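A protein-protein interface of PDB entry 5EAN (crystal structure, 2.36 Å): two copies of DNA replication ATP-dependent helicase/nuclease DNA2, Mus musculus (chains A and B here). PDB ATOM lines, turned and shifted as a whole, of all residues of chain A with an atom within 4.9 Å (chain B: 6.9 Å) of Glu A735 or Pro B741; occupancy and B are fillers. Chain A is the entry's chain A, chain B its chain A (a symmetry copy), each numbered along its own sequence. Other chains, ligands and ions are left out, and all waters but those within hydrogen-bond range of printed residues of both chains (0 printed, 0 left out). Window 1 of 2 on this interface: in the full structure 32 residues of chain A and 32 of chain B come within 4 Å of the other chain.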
ATOM      1  N   ALA A 731       8.035  -3.682 -18.306  1.00  0.00           N
ATOM      2  CA  ALA A 731       8.814  -4.174 -19.471  1.00  0.00           C
ATOM      3  C   ALA A 731       8.526  -5.629 -19.830  1.00  0.00           C
ATOM      4  O   ALA A 731       8.340  -5.914 -21.002  1.00  0.00           O
ATOM      5  CB  ALA A 731      10.307  -3.943 -19.303  1.00  0.00           C
ATOM      6  N   HIS A 732       8.458  -6.534 -18.849  1.00  0.00           N
ATOM      7  CA  HIS A 732       8.002  -7.922 -19.117  1.00  0.00           C
ATOM      8  C   HIS A 732       6.587  -8.031 -19.652  1.00  0.00           C
ATOM      9  O   HIS A 732       6.343  -8.854 -20.535  1.00  0.00           O
ATOM     10  CB  HIS A 732       8.192  -8.872 -17.927  1.00  0.00           C
ATOM     11  CG  HIS A 732       9.601  -9.337 -17.769  1.00  0.00           C
ATOM     12  ND1 HIS A 732      10.132  -9.720 -16.555  1.00  0.00           N
ATOM     13  CD2 HIS A 732      10.618  -9.419 -18.664  1.00  0.00           C
ATOM     14  CE1 HIS A 732      11.406 -10.052 -16.713  1.00  0.00           C
ATOM     15  NE2 HIS A 732      11.727  -9.872 -17.982  1.00  0.00           N
ATOM     16  N   LEU A 733       5.663  -7.203 -19.161  1.00  0.00           N
ATOM     17  CA  LEU A 733       4.324  -7.188 -19.762  1.00  0.00           C
ATOM     18  C   LEU A 733       4.347  -6.753 -21.206  1.00  0.00           C
ATOM     19  O   LEU A 733       3.702  -7.378 -22.066  1.00  0.00           O
ATOM     20  CB  LEU A 733       3.309  -6.369 -18.940  1.00  0.00           C
ATOM     21  CG  LEU A 733       1.820  -6.612 -19.276  1.00  0.00           C
ATOM     22  CD1 LEU A 733       1.361  -8.077 -19.096  1.00  0.00           C
ATOM     23  CD2 LEU A 733       0.928  -5.665 -18.486  1.00  0.00           C
ATOM     24  N   GLU A 734       5.080  -5.672 -21.481  1.00  0.00           N
ATOM     25  CA  GLU A 734       5.233  -5.200 -22.851  1.00  0.00           C
ATOM     26  C   GLU A 734       5.798  -6.297 -23.713  1.00  0.00           C
ATOM     27  O   GLU A 734       5.297  -6.548 -24.784  1.00  0.00           O
ATOM     28  CB  GLU A 734       6.179  -4.016 -22.927  1.00  0.00           C
ATOM     29  CG  GLU A 734       5.490  -2.698 -22.778  1.00  0.00           C
ATOM     30  CD  GLU A 734       6.384  -1.550 -23.193  1.00  0.00           C
ATOM     31  OE1 GLU A 734       6.868  -0.840 -22.295  1.00  0.00           O
ATOM     32  OE2 GLU A 734       6.600  -1.365 -24.415  1.00  0.00           O
ATOM     33  N   GLU A 735       6.853  -6.936 -23.233  1.00  0.00           N
ATOM     34  CA  GLU A 735       7.489  -8.037 -23.927  1.00  0.00           C
ATOM     35  C   GLU A 735       6.469  -9.109 -24.341  1.00  0.00           C
ATOM     36  O   GLU A 735       6.484  -9.574 -25.477  1.00  0.00           O
ATOM     37  CB  GLU A 735       8.581  -8.628 -23.046  1.00  0.00           C
ATOM     38  CG  GLU A 735       9.715  -9.260 -23.808  1.00  0.00           C
ATOM     39  CD  GLU A 735      10.746  -9.914 -22.906  1.00  0.00           C
ATOM     40  OE1 GLU A 735      10.883  -9.516 -21.724  1.00  0.00           O
ATOM     41  OE2 GLU A 735      11.432 -10.837 -23.395  1.00  0.00           O
ATOM     42  N   LEU A 736       5.543  -9.444 -23.456  1.00  0.00           N
ATOM     43  CA  LEU A 736       4.531 -10.406 -23.800  1.00  0.00           C
ATOM     44  C   LEU A 736       3.599  -9.902 -24.910  1.00  0.00           C
ATOM     45  O   LEU A 736       3.349 -10.628 -25.885  1.00  0.00           O
ATOM     46  CB  LEU A 736       3.767 -10.862 -22.563  1.00  0.00           C
ATOM     47  CG  LEU A 736       2.561 -11.769 -22.820  1.00  0.00           C
ATOM     48  CD1 LEU A 736       2.981 -13.134 -23.352  1.00  0.00           C
ATOM     49  CD2 LEU A 736       1.731 -11.885 -21.549  1.00  0.00           C
ATOM     50  N   TYR A 737       3.124  -8.667 -24.785  1.00  0.00           N
ATOM     51  CA  TYR A 737       2.299  -8.030 -25.811  1.00  0.00           C
ATOM     52  C   TYR A 737       3.021  -7.916 -27.169  1.00  0.00           C
ATOM     53  O   TYR A 737       2.388  -8.012 -28.205  1.00  0.00           O
ATOM     54  CB  TYR A 737       1.758  -6.651 -25.347  1.00  0.00           C
ATOM     55  CG  TYR A 737       0.797  -6.673 -24.134  1.00  0.00           C
ATOM     56  CD1 TYR A 737       0.145  -7.870 -23.710  1.00  0.00           C
ATOM     57  CD2 TYR A 737       0.501  -5.482 -23.430  1.00  0.00           C
ATOM     58  CE1 TYR A 737      -0.712  -7.895 -22.616  1.00  0.00           C
ATOM     59  CE2 TYR A 737      -0.384  -5.487 -22.353  1.00  0.00           C
ATOM     60  CZ  TYR A 737      -0.982  -6.695 -21.939  1.00  0.00           C
ATOM     61  OH  TYR A 737      -1.853  -6.686 -20.861  1.00  0.00           O
ATOM     62  N   ASN A 738       4.332  -7.721 -27.183  1.00  0.00           N
ATOM     63  CA  ASN A 738       5.033  -7.639 -28.468  1.00  0.00           C
ATOM     64  C   ASN A 738       5.565  -8.958 -28.977  1.00  0.00           C
ATOM     65  O   ASN A 738       6.241  -8.972 -30.000  1.00  0.00           O
ATOM     66  CB  ASN A 738       6.195  -6.675 -28.377  1.00  0.00           C
ATOM     67  CG  ASN A 738       5.759  -5.281 -27.992  1.00  0.00           C
ATOM     68  OD1 ASN A 738       4.737  -4.783 -28.448  1.00  0.00           O
ATOM     69  ND2 ASN A 738       6.539  -4.646 -27.159  1.00  0.00           N
ATOM     70  N   SER A 739       5.299 -10.060 -28.278  1.00  0.00           N
ATOM     71  CA  SER A 739       6.012 -11.296 -28.613  1.00  0.00           C
ATOM     72  C   SER A 739       5.414 -12.009 -29.830  1.00  0.00           C
ATOM     73  O   SER A 739       6.062 -12.846 -30.411  1.00  0.00           O
ATOM     74  CB  SER A 739       6.147 -12.239 -27.406  1.00  0.00           C
ATOM     75  OG  SER A 739       4.883 -12.608 -26.877  1.00  0.00           O
ATOM     76  N   SER B 670      17.972  -6.753 -15.538  1.00  0.00           N
ATOM     77  CA  SER B 670      17.287  -7.671 -16.449  1.00  0.00           C
ATOM     78  C   SER B 670      16.472  -8.761 -15.709  1.00  0.00           C
ATOM     79  O   SER B 670      15.294  -8.947 -16.013  1.00  0.00           O
ATOM     80  CB  SER B 670      18.303  -8.294 -17.401  1.00  0.00           C
ATOM     81  OG  SER B 670      17.761  -9.405 -18.091  1.00  0.00           O
ATOM     82  N   GLY B 673      13.374  -7.562 -14.487  1.00  0.00           N
ATOM     83  CA  GLY B 673      12.422  -7.189 -15.533  1.00  0.00           C
ATOM     84  C   GLY B 673      12.364  -5.712 -15.895  1.00  0.00           C
ATOM     85  O   GLY B 673      11.341  -5.227 -16.379  1.00  0.00           O
ATOM     86  N   PHE B 674      13.453  -4.992 -15.664  1.00  0.00           N
ATOM     87  CA  PHE B 674      13.544  -3.594 -16.078  1.00  0.00           C
ATOM     88  C   PHE B 674      14.028  -3.584 -17.523  1.00  0.00           C
ATOM     89  O   PHE B 674      14.699  -4.540 -17.961  1.00  0.00           O
ATOM     90  CB  PHE B 674      14.578  -2.881 -15.229  1.00  0.00           C
ATOM     91  CG  PHE B 674      14.141  -2.603 -13.823  1.00  0.00           C
ATOM     92  CD1 PHE B 674      13.019  -1.818 -13.556  1.00  0.00           C
ATOM     93  CD2 PHE B 674      14.879  -3.086 -12.734  1.00  0.00           C
ATOM     94  CE1 PHE B 674      12.627  -1.528 -12.225  1.00  0.00           C
ATOM     95  CE2 PHE B 674      14.493  -2.805 -11.404  1.00  0.00           C
ATOM     96  CZ  PHE B 674      13.367  -2.012 -11.153  1.00  0.00           C
ATOM     97  N   SER B 675      13.712  -2.525 -18.262  1.00  0.00           N
ATOM     98  CA  SER B 675      14.354  -2.291 -19.548  1.00  0.00           C
ATOM     99  C   SER B 675      15.529  -1.363 -19.306  1.00  0.00           C
ATOM    100  O   SER B 675      15.478  -0.514 -18.404  1.00  0.00           O
ATOM    101  CB  SER B 675      13.388  -1.714 -20.590  1.00  0.00           C
ATOM    102  OG  SER B 675      12.724  -0.584 -20.083  1.00  0.00           O
ATOM    103  N   VAL B 676      16.599  -1.564 -20.079  1.00  0.00           N
ATOM    104  CA  VAL B 676      17.899  -0.903 -19.857  1.00  0.00           C
ATOM    105  C   VAL B 676      18.472  -0.386 -21.168  1.00  0.00           C
ATOM    106  O   VAL B 676      18.502  -1.111 -22.174  1.00  0.00           O
ATOM    107  CB  VAL B 676      18.940  -1.846 -19.189  1.00  0.00           C
ATOM    108  CG1 VAL B 676      20.209  -1.097 -18.805  1.00  0.00           C
ATOM    109  CG2 VAL B 676      18.374  -2.455 -17.929  1.00  0.00           C
ATOM    110  N   LEU B 677      18.886   0.873 -21.149  1.00  0.00           N
ATOM    111  CA  LEU B 677      19.583   1.500 -22.263  1.00  0.00           C
ATOM    112  C   LEU B 677      21.037   1.630 -21.854  1.00  0.00           C
ATOM    113  O   LEU B 677      21.379   2.406 -20.945  1.00  0.00           O
ATOM    114  CB  LEU B 677      18.982   2.887 -22.590  1.00  0.00           C
ATOM    115  CG  LEU B 677      19.734   3.712 -23.631  1.00  0.00           C
ATOM    116  CD1 LEU B 677      19.848   2.974 -24.954  1.00  0.00           C
ATOM    117  CD2 LEU B 677      19.079   5.085 -23.854  1.00  0.00           C
ATOM    118  N   GLY B 699      20.255 -11.571 -23.403  1.00  0.00           N
ATOM    119  CA  GLY B 699      19.921 -11.004 -24.700  1.00  0.00           C
ATOM    120  C   GLY B 699      19.926  -9.489 -24.666  1.00  0.00           C
ATOM    121  O   GLY B 699      19.548  -8.853 -23.655  1.00  0.00           O
ATOM    122  N   PHE B 700      20.356  -8.917 -25.786  1.00  0.00           N
ATOM    123  CA  PHE B 700      20.396  -7.472 -26.015  1.00  0.00           C
ATOM    124  C   PHE B 700      20.357  -7.202 -27.511  1.00  0.00           C
ATOM    125  O   PHE B 700      20.717  -8.062 -28.328  1.00  0.00           O
ATOM    126  CB  PHE B 700      21.661  -6.827 -25.422  1.00  0.00           C
ATOM    127  CG  PHE B 700      22.951  -7.535 -25.798  1.00  0.00           C
ATOM    128  CD1 PHE B 700      23.632  -7.220 -26.985  1.00  0.00           C
ATOM    129  CD2 PHE B 700      23.484  -8.546 -24.969  1.00  0.00           C
ATOM    130  CE1 PHE B 700      24.814  -7.896 -27.329  1.00  0.00           C
ATOM    131  CE2 PHE B 700      24.671  -9.203 -25.314  1.00  0.00           C
ATOM    132  CZ  PHE B 700      25.332  -8.879 -26.493  1.00  0.00           C
ATOM    133  N   LEU B 701      19.920  -5.992 -27.865  1.00  0.00           N
ATOM    134  CA  LEU B 701      20.042  -5.528 -29.222  1.00  0.00           C
ATOM    135  C   LEU B 701      21.108  -4.453 -29.320  1.00  0.00           C
ATOM    136  O   LEU B 701      21.146  -3.539 -28.495  1.00  0.00           O
ATOM    137  CB  LEU B 701      18.699  -5.033 -29.742  1.00  0.00           C
ATOM    138  CG  LEU B 701      18.661  -4.394 -31.136  1.00  0.00           C
ATOM    139  CD1 LEU B 701      18.947  -5.439 -32.202  1.00  0.00           C
ATOM    140  CD2 LEU B 701      17.324  -3.655 -31.369  1.00  0.00           C
ATOM    141  N   TYR B 737      13.018  -4.715 -32.786  1.00  0.00           N
ATOM    142  CA  TYR B 737      13.122  -3.637 -31.804  1.00  0.00           C
ATOM    143  C   TYR B 737      12.511  -4.014 -30.439  1.00  0.00           C
ATOM    144  O   TYR B 737      13.005  -3.585 -29.411  1.00  0.00           O
ATOM    145  CB  TYR B 737      12.526  -2.306 -32.336  1.00  0.00           C
ATOM    146  CG  TYR B 737      13.237  -1.689 -33.564  1.00  0.00           C
ATOM    147  CD1 TYR B 737      14.555  -2.079 -33.948  1.00  0.00           C
ATOM    148  CD2 TYR B 737      12.607  -0.675 -34.324  1.00  0.00           C
ATOM    149  CE1 TYR B 737      15.193  -1.532 -35.055  1.00  0.00           C
ATOM    150  CE2 TYR B 737      13.250  -0.093 -35.416  1.00  0.00           C
ATOM    151  CZ  TYR B 737      14.538  -0.529 -35.788  1.00  0.00           C
ATOM    152  OH  TYR B 737      15.161   0.052 -36.881  1.00  0.00           O
ATOM    153  N   ASN B 738      11.453  -4.813 -30.410  1.00  0.00           N
ATOM    154  CA  ASN B 738      10.881  -5.200 -29.117  1.00  0.00           C
ATOM    155  C   ASN B 738      11.440  -6.481 -28.542  1.00  0.00           C
ATOM    156  O   ASN B 738      10.958  -6.928 -27.507  1.00  0.00           O
ATOM    157  CB  ASN B 738       9.381  -5.359 -29.228  1.00  0.00           C
ATOM    158  CG  ASN B 738       8.698  -4.090 -29.681  1.00  0.00           C
ATOM    159  OD1 ASN B 738       9.050  -2.993 -29.265  1.00  0.00           O
ATOM    160  ND2 ASN B 738       7.714  -4.238 -30.526  1.00  0.00           N
ATOM    161  N   SER B 739      12.425  -7.091 -29.197  1.00  0.00           N
ATOM    162  CA  SER B 739      12.802  -8.449 -28.797  1.00  0.00           C
ATOM    163  C   SER B 739      13.708  -8.470 -27.561  1.00  0.00           C
ATOM    164  O   SER B 739      13.840  -9.492 -26.933  1.00  0.00           O
ATOM    165  CB  SER B 739      13.402  -9.258 -29.959  1.00  0.00           C
ATOM    166  OG  SER B 739      14.560  -8.636 -30.495  1.00  0.00           O
ATOM    167  N   HIS B 740      14.310  -7.341 -27.206  1.00  0.00           N
ATOM    168  CA  HIS B 740      15.145  -7.292 -26.010  1.00  0.00           C
ATOM    169  C   HIS B 740      14.959  -6.022 -25.217  1.00  0.00           C
ATOM    170  O   HIS B 740      15.067  -4.933 -25.770  1.00  0.00           O
ATOM    171  CB  HIS B 740      16.636  -7.511 -26.326  1.00  0.00           C
ATOM    172  CG  HIS B 740      16.927  -8.869 -26.872  1.00  0.00           C
ATOM    173  ND1 HIS B 740      17.228  -9.079 -28.200  1.00  0.00           N
ATOM    174  CD2 HIS B 740      16.881 -10.094 -26.292  1.00  0.00           C
ATOM    175  CE1 HIS B 740      17.406 -10.374 -28.406  1.00  0.00           C
ATOM    176  NE2 HIS B 740      17.189 -11.012 -27.268  1.00  0.00           N
ATOM    177  N   PRO B 741      14.680  -6.170 -23.912  1.00  0.00           N
ATOM    178  CA  PRO B 741      14.578  -5.099 -22.954  1.00  0.00           C
ATOM    179  C   PRO B 741      15.878  -4.312 -22.850  1.00  0.00           C
ATOM    180  O   PRO B 741      15.870  -3.173 -22.393  1.00  0.00           O
ATOM    181  CB  PRO B 741      14.338  -5.858 -21.658  1.00  0.00           C
ATOM    182  CG  PRO B 741      13.589  -7.076 -22.090  1.00  0.00           C
ATOM    183  CD  PRO B 741      14.345  -7.469 -23.298  1.00  0.00           C
ATOM    184  N   ILE B 742      16.984  -4.924 -23.265  1.00  0.00           N
ATOM    185  CA  ILE B 742      18.294  -4.286 -23.222  1.00  0.00           C
ATOM    186  C   ILE B 742      18.706  -3.817 -24.602  1.00  0.00           C
ATOM    187  O   ILE B 742      18.847  -4.617 -25.521  1.00  0.00           O
ATOM    188  CB  ILE B 742      19.348  -5.221 -22.627  1.00  0.00           C
ATOM    189  CG1 ILE B 742      18.860  -5.710 -21.240  1.00  0.00           C
ATOM    190  CG2 ILE B 742      20.720  -4.524 -22.563  1.00  0.00           C
ATOM    191  CD1 ILE B 742      19.644  -6.875 -20.687  1.00  0.00           C
ATOM    192  N   VAL B 743      18.886  -2.507 -24.736  1.00  0.00           N
ATOM    193  CA  VAL B 743      19.307  -1.903 -25.989  1.00  0.00           C
ATOM    194  C   VAL B 743      20.627  -1.157 -25.775  1.00  0.00           C
ATOM    195  O   VAL B 743      20.753  -0.323 -24.860  1.00  0.00           O
ATOM    196  CB  VAL B 743      18.207  -0.972 -26.569  1.00  0.00           C
ATOM    197  CG1 VAL B 743      18.728  -0.253 -27.795  1.00  0.00           C
ATOM    198  CG2 VAL B 743      16.961  -1.773 -26.950  1.00  0.00           C
ATOM    199  N   LYS B 758      10.279   4.345 -27.753  1.00  0.00           N
ATOM    200  CA  LYS B 758      10.530   3.590 -26.520  1.00  0.00           C
ATOM    201  C   LYS B 758      11.130   4.465 -25.429  1.00  0.00           C
ATOM    202  O   LYS B 758      11.839   5.442 -25.721  1.00  0.00           O
ATOM    203  CB  LYS B 758      11.511   2.442 -26.797  1.00  0.00           C
ATOM    204  CG  LYS B 758      10.864   1.195 -27.341  1.00  0.00           C
ATOM    205  CD  LYS B 758      11.890   0.077 -27.501  1.00  0.00           C
ATOM    206  CE  LYS B 758      11.417  -1.194 -26.817  1.00  0.00           C
ATOM    207  NZ  LYS B 758      10.013  -1.576 -27.180  1.00  0.00           N
ATOM    208  N   PHE B 760      13.025   3.857 -21.333  1.00  0.00           N
ATOM    209  CA  PHE B 760      13.656   2.813 -20.584  1.00  0.00           C
ATOM    210  C   PHE B 760      13.537   3.087 -19.098  1.00  0.00           C
ATOM    211  O   PHE B 760      13.496   4.251 -18.674  1.00  0.00           O
ATOM    212  CB  PHE B 760      15.109   2.718 -21.029  1.00  0.00           C
ATOM    213  CG  PHE B 760      15.265   2.286 -22.458  1.00  0.00           C
ATOM    214  CD1 PHE B 760      15.240   3.222 -23.502  1.00  0.00           C
ATOM    215  CD2 PHE B 760      15.448   0.924 -22.776  1.00  0.00           C
ATOM    216  CE1 PHE B 760      15.383   2.805 -24.833  1.00  0.00           C
ATOM    217  CE2 PHE B 760      15.596   0.513 -24.093  1.00  0.00           C
ATOM    218  CZ  PHE B 760      15.550   1.457 -25.124  1.00  0.00           C
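ND2 of Asn A738 is in hydrogen-bond range of O of Glu A734.
The backbone NH of Val B676 sits at hydrogen-bond distance from the backbone carbonyl oxygen of Pro B741.
The side-chain amide oxygen (OD1) of Asn B738 sits at hydrogen-bond distance from the side-chain amino group (NZ) of Lys B758 (2.7 Å).
Ala A731 touches Gly B673 (CB to O, 3.4 Å).
N of Ser B675 touches CB of Ala A731, at 3.8 Å.
His A732 touches Gly B673.
OE1 of Glu A735 touches CG of Pro B741, at 3.7 Å.
Asn A738 touches Asn B738 (ND2 to CG, 3.4 Å).
Glu A735 touches just one residue of chain B: Pro B741.
Pro B741 touches just one residue of chain A: Glu A735 (3.7 Å).
Of the printed residues of chain A, Gly B673 touches Ala A731 (3.4 Å) and His A732 (3.3 Å).
Of the printed residues of chain B, Ala A731 touches Gly B673 and Ser B675.
Of the printed residues of chain A, Asn B738 touches Asn A738 (3.4 Å).
Of the printed residues of chain B, His A732 touches Gly B673 (3.3 Å).
Phe B674 touches none of the printed residues of chain A.
The nearest residue of chain B that does not touch Glu A735 is Ser B739 (4.5 Å).
The nearest printed residue of chain A that does not touch Pro B741 is Ala A731 (5.0 Å).
Hydrophobic or aromatic side chains of chain B within 4 Å of the printed part of chain A: Pro B741.
Hydrophobic or aromatic side chains of chain A within 4 Å of the printed part of chain B: Ala A731 and His A732.
Asn B738 touches its own counterpart, Asn A738.
3 positions are printed for both chains.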
